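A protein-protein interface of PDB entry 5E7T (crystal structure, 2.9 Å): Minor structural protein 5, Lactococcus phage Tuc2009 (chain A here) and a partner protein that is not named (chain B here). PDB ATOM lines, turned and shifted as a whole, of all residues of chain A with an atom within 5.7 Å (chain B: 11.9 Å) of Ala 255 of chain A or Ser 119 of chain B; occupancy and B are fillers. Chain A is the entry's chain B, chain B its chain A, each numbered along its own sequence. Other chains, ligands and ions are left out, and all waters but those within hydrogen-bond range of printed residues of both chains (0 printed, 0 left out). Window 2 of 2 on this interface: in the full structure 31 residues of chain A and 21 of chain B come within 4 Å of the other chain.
O of Thr 283 of chain A sits at hydrogen-bond distance from N of Gly 256 of chain A, 3.1 Å away. The side-chain hydroxyl (OG1) of Thr 118 of chain B lies within hydrogen-bond range of the side-chain hydroxyl (OG) of Ser 121 of chain B, at 3.0 Å. The side-chain hydroxyl of Thr 282 of chain A is in hydrogen-bond range of the backbone carbonyl oxygen of Lys 254 of chain A (2.6 Å). The backbone NH (N) of Thr 257 of chain A lies within hydrogen-bond range of the side-chain hydroxyl (OG1) of Thr 282 of chain A (2.9 Å). The backbone NH (N) of Thr 120 of chain B sits close to the side-chain hydroxyl (OG1) of Thr 118 of chain B. The backbone NH of Gly 256 of chain A lies within hydrogen-bond range of the side-chain hydroxyl of Thr 282 of chain A, at 3.1 Å.
Hydrophobic or aromatic side chains of chain A that line the printed part of chain B: Leu 253 and Ala 255. Among the printed residues, 9 pairs touch across the chains.
The backbone carbonyl oxygen (O) of Thr 120 of chain B is in hydrogen-bond range of the backbone NH (N) of Leu 253 of chain A (2.9 Å). N of Ser 119 of chain B lies within hydrogen-bond range of OG1 of Thr 283 of chain A. The backbone carbonyl oxygen (O) of Ser 119 of chain B lies within hydrogen-bond range of the backbone NH (N) of Ala 255 of chain A (3.2 Å). The backbone carbonyl oxygen (O) of Lys 254 of chain A lies close to the backbone carbonyl oxygen (O) of Ser 119 of chain B. The backbone carbonyl oxygen (O) of Thr 118 of chain B sits at hydrogen-bond distance from the backbone NH (N) of Thr 283 of chain A (3.4 Å).
Of chain B, only Ser 119 comes within 4 Å of Ala 255 of chain A. Of chain A, only Leu 253, Lys 254, Ala 255, Thr 282 and Thr 283 come within 4 Å of Ser 119 of chain B. Leu 253 of chain A touches just these residues of chain B: Ser 119, Thr 120 and Ser 121. Lys 254 of chain A touches one residue of chain B. No residue of chain B comes within 4 Å of Gly 256 of chain A. Of chain B, only Thr 118 (3.2 Å) and Ser 119 (3.2 Å) come within 4 Å of Thr 283 of chain A. Leu 284 of chain A touches none of the printed residues of chain B. No residue of chain B comes within 4 Å of Pro 285 of chain A. Of the printed residues of chain A, Thr 120 of chain B touches Leu 253 (2.9 Å). Printed residues of chain A within 4 Å of Ser 121 of chain B: Leu 253 (3.9 Å). Of the printed residues of chain A, Thr 118 of chain B touches Thr 282 (3.4 Å) and Thr 283 (3.2 Å).
O of Ser 119 of chain B touches O of Leu 253 of chain A, 3.8 Å away. CA of Ser 121 of chain B touches CD1 of Leu 253 of chain A, 3.9 Å away. CB of Thr 282 of chain A touches O of Thr 118 of chain B, at 3.4 Å. Thr 282 of chain A touches Ser 119 of chain B (CB to O, 3.4 Å).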
ATOM      1  N   LEU A 253     -31.262  15.310 -21.683  1.00  0.00           N
ATOM      2  CA  LEU A 253     -30.214  16.206 -22.167  1.00  0.00           C
ATOM      3  C   LEU A 253     -28.888  15.473 -22.011  1.00  0.00           C
ATOM      4  O   LEU A 253     -28.815  14.502 -21.249  1.00  0.00           O
ATOM      5  CB  LEU A 253     -30.182  17.537 -21.372  1.00  0.00           C
ATOM      6  CG  LEU A 253     -31.493  18.326 -21.207  1.00  0.00           C
ATOM      7  CD1 LEU A 253     -31.293  19.499 -20.288  1.00  0.00           C
ATOM      8  CD2 LEU A 253     -32.059  18.792 -22.543  1.00  0.00           C
ATOM      9  N   LYS A 254     -27.844  15.916 -22.735  1.00  0.00           N
ATOM     10  CA  LYS A 254     -26.512  15.313 -22.630  1.00  0.00           C
ATOM     11  C   LYS A 254     -25.644  16.191 -21.730  1.00  0.00           C
ATOM     12  O   LYS A 254     -25.835  17.408 -21.704  1.00  0.00           O
ATOM     13  CB  LYS A 254     -25.874  15.084 -24.016  1.00  0.00           C
ATOM     14  CG  LYS A 254     -26.787  14.377 -25.042  1.00  0.00           C
ATOM     15  CD  LYS A 254     -27.186  12.940 -24.660  1.00  0.00           C
ATOM     16  CE  LYS A 254     -28.512  12.514 -25.262  1.00  0.00           C
ATOM     17  NZ  LYS A 254     -29.123  11.382 -24.506  1.00  0.00           N
ATOM     18  N   ALA A 255     -24.734  15.568 -20.957  1.00  0.00           N
ATOM     19  CA  ALA A 255     -23.829  16.233 -20.008  1.00  0.00           C
ATOM     20  C   ALA A 255     -22.905  17.259 -20.632  1.00  0.00           C
ATOM     21  O   ALA A 255     -22.532  17.134 -21.795  1.00  0.00           O
ATOM     22  CB  ALA A 255     -23.014  15.208 -19.252  1.00  0.00           C
ATOM     23  N   GLY A 256     -22.547  18.259 -19.838  1.00  0.00           N
ATOM     24  CA  GLY A 256     -21.645  19.336 -20.220  1.00  0.00           C
ATOM     25  C   GLY A 256     -21.930  20.038 -21.533  1.00  0.00           C
ATOM     26  O   GLY A 256     -20.985  20.474 -22.199  1.00  0.00           O
ATOM     27  N   THR A 257     -23.219  20.147 -21.934  1.00  0.00           N
ATOM     28  CA  THR A 257     -23.548  20.865 -23.162  1.00  0.00           C
ATOM     29  C   THR A 257     -24.427  22.081 -22.891  1.00  0.00           C
ATOM     30  O   THR A 257     -25.288  22.035 -22.009  1.00  0.00           O
ATOM     31  CB  THR A 257     -24.118  19.988 -24.268  1.00  0.00           C
ATOM     32  OG1 THR A 257     -25.509  20.164 -24.276  1.00  0.00           O
ATOM     33  CG2 THR A 257     -23.771  18.510 -24.147  1.00  0.00           C
ATOM     34  N   THR A 282     -25.697  21.967 -18.935  1.00  0.00           N
ATOM     35  CA  THR A 282     -25.806  20.778 -18.084  1.00  0.00           C
ATOM     36  C   THR A 282     -24.465  20.588 -17.383  1.00  0.00           C
ATOM     37  O   THR A 282     -23.421  20.957 -17.935  1.00  0.00           O
ATOM     38  CB  THR A 282     -26.178  19.517 -18.900  1.00  0.00           C
ATOM     39  OG1 THR A 282     -25.364  19.424 -20.067  1.00  0.00           O
ATOM     40  CG2 THR A 282     -27.630  19.474 -19.285  1.00  0.00           C
ATOM     41  N   THR A 283     -24.490  20.037 -16.170  1.00  0.00           N
ATOM     42  CA  THR A 283     -23.266  19.805 -15.415  1.00  0.00           C
ATOM     43  C   THR A 283     -22.512  18.603 -15.984  1.00  0.00           C
ATOM     44  O   THR A 283     -23.073  17.850 -16.780  1.00  0.00           O
ATOM     45  CB  THR A 283     -23.569  19.721 -13.915  1.00  0.00           C
ATOM     46  OG1 THR A 283     -24.640  18.802 -13.707  1.00  0.00           O
ATOM     47  CG2 THR A 283     -23.930  21.073 -13.325  1.00  0.00           C
ATOM     48  N   LEU A 284     -21.227  18.458 -15.633  1.00  0.00           N
ATOM     49  CA  LEU A 284     -20.439  17.315 -16.093  1.00  0.00           C
ATOM     50  C   LEU A 284     -20.413  16.228 -15.012  1.00  0.00           C
ATOM     51  O   LEU A 284     -20.286  16.572 -13.834  1.00  0.00           O
ATOM     52  CB  LEU A 284     -19.022  17.733 -16.492  1.00  0.00           C
ATOM     53  CG  LEU A 284     -18.830  17.947 -17.982  1.00  0.00           C
ATOM     54  CD1 LEU A 284     -17.765  18.989 -18.252  1.00  0.00           C
ATOM     55  CD2 LEU A 284     -18.552  16.622 -18.713  1.00  0.00           C
ATOM     56  N   PRO A 285     -20.558  14.926 -15.342  1.00  0.00           N
ATOM     57  CA  PRO A 285     -20.530  13.908 -14.279  1.00  0.00           C
ATOM     58  C   PRO A 285     -19.101  13.485 -13.859  1.00  0.00           C
ATOM     59  O   PRO A 285     -18.135  13.714 -14.605  1.00  0.00           O
ATOM     60  CB  PRO A 285     -21.373  12.759 -14.866  1.00  0.00           C
ATOM     61  CG  PRO A 285     -21.569  13.090 -16.354  1.00  0.00           C
ATOM     62  CD  PRO A 285     -20.726  14.294 -16.666  1.00  0.00           C
ATOM     63  N   SER B 115     -33.569  26.217 -13.256  1.00  0.00           N
ATOM     64  CA  SER B 115     -33.309  25.706 -11.909  1.00  0.00           C
ATOM     65  C   SER B 115     -33.168  24.192 -11.966  1.00  0.00           C
ATOM     66  O   SER B 115     -33.432  23.604 -13.018  1.00  0.00           O
ATOM     67  CB  SER B 115     -34.461  26.082 -10.983  1.00  0.00           C
ATOM     68  OG  SER B 115     -35.725  25.884 -11.600  1.00  0.00           O
ATOM     69  N   ASP B 116     -32.754  23.554 -10.841  1.00  0.00           N
ATOM     70  CA  ASP B 116     -32.590  22.097 -10.723  1.00  0.00           C
ATOM     71  C   ASP B 116     -31.844  21.471 -11.934  1.00  0.00           C
ATOM     72  O   ASP B 116     -32.297  20.463 -12.488  1.00  0.00           O
ATOM     73  CB  ASP B 116     -33.960  21.416 -10.476  1.00  0.00           C
ATOM     74  CG  ASP B 116     -34.663  21.835  -9.196  1.00  0.00           C
ATOM     75  OD1 ASP B 116     -35.358  22.878  -9.213  1.00  0.00           O
ATOM     76  OD2 ASP B 116     -34.552  21.095  -8.189  1.00  0.00           O
ATOM     77  N   VAL B 117     -30.713  22.089 -12.350  1.00  0.00           N
ATOM     78  CA  VAL B 117     -29.935  21.634 -13.525  1.00  0.00           C
ATOM     79  C   VAL B 117     -28.903  20.560 -13.123  1.00  0.00           C
ATOM     80  O   VAL B 117     -28.109  20.755 -12.200  1.00  0.00           O
ATOM     81  CB  VAL B 117     -29.329  22.784 -14.407  1.00  0.00           C
ATOM     82  CG1 VAL B 117     -29.108  24.058 -13.609  1.00  0.00           C
ATOM     83  CG2 VAL B 117     -28.056  22.369 -15.139  1.00  0.00           C
ATOM     84  N   THR B 118     -28.972  19.406 -13.817  1.00  0.00           N
ATOM     85  CA  THR B 118     -28.105  18.240 -13.640  1.00  0.00           C
ATOM     86  C   THR B 118     -27.424  17.932 -14.983  1.00  0.00           C
ATOM     87  O   THR B 118     -27.592  18.688 -15.941  1.00  0.00           O
ATOM     88  CB  THR B 118     -28.914  17.026 -13.130  1.00  0.00           C
ATOM     89  OG1 THR B 118     -29.647  16.441 -14.200  1.00  0.00           O
ATOM     90  CG2 THR B 118     -29.840  17.363 -11.981  1.00  0.00           C
ATOM     91  N   SER B 119     -26.677  16.815 -15.063  1.00  0.00           N
ATOM     92  CA  SER B 119     -26.008  16.420 -16.297  1.00  0.00           C
ATOM     93  C   SER B 119     -27.000  16.011 -17.382  1.00  0.00           C
ATOM     94  O   SER B 119     -26.726  16.215 -18.557  1.00  0.00           O
ATOM     95  CB  SER B 119     -25.013  15.294 -16.034  1.00  0.00           C
ATOM     96  OG  SER B 119     -25.641  14.145 -15.490  1.00  0.00           O
ATOM     97  N   THR B 120     -28.161  15.474 -16.992  1.00  0.00           N
ATOM     98  CA  THR B 120     -29.173  14.961 -17.918  1.00  0.00           C
ATOM     99  C   THR B 120     -30.487  15.797 -17.955  1.00  0.00           C
ATOM    100  O   THR B 120     -31.318  15.544 -18.828  1.00  0.00           O
ATOM    101  CB  THR B 120     -29.431  13.451 -17.614  1.00  0.00           C
ATOM    102  OG1 THR B 120     -30.577  12.973 -18.327  1.00  0.00           O
ATOM    103  CG2 THR B 120     -29.610  13.152 -16.113  1.00  0.00           C
ATOM    104  N   SER B 121     -30.678  16.781 -17.052  1.00  0.00           N
ATOM    105  CA  SER B 121     -31.929  17.553 -17.016  1.00  0.00           C
ATOM    106  C   SER B 121     -31.812  18.993 -16.480  1.00  0.00           C
ATOM    107  O   SER B 121     -30.764  19.386 -15.967  1.00  0.00           O
ATOM    108  CB  SER B 121     -32.951  16.803 -16.164  1.00  0.00           C
ATOM    109  OG  SER B 121     -32.559  16.792 -14.798  1.00  0.00           O
ATOM    110  N   ALA B 122     -32.928  19.754 -16.554  1.00  0.00           N
ATOM    111  CA  ALA B 122     -33.098  21.115 -16.016  1.00  0.00           C
ATOM    112  C   ALA B 122     -34.582  21.451 -15.955  1.00  0.00           C
ATOM    113  O   ALA B 122     -35.384  20.809 -16.636  1.00  0.00           O
ATOM    114  CB  ALA B 122     -32.362  22.144 -16.857  1.00  0.00           C
ATOM    115  N   LYS B 123     -34.955  22.432 -15.123  1.00  0.00           N
ATOM    116  CA  LYS B 123     -36.339  22.852 -14.958  1.00  0.00           C
ATOM    117  C   LYS B 123     -36.451  24.278 -15.434  1.00  0.00           C
ATOM    118  O   LYS B 123     -35.677  25.147 -15.017  1.00  0.00           O
ATOM    119  CB  LYS B 123     -36.794  22.716 -13.490  1.00  0.00           C
ATOM    120  CG  LYS B 123     -38.306  22.849 -13.285  1.00  0.00           C
ATOM    121  CD  LYS B 123     -38.772  22.363 -11.918  1.00  0.00           C
ATOM    122  CE  LYS B 123     -38.967  23.498 -10.939  1.00  0.00           C
ATOM    123  NZ  LYS B 123     -37.677  23.986 -10.375  1.00  0.00           N
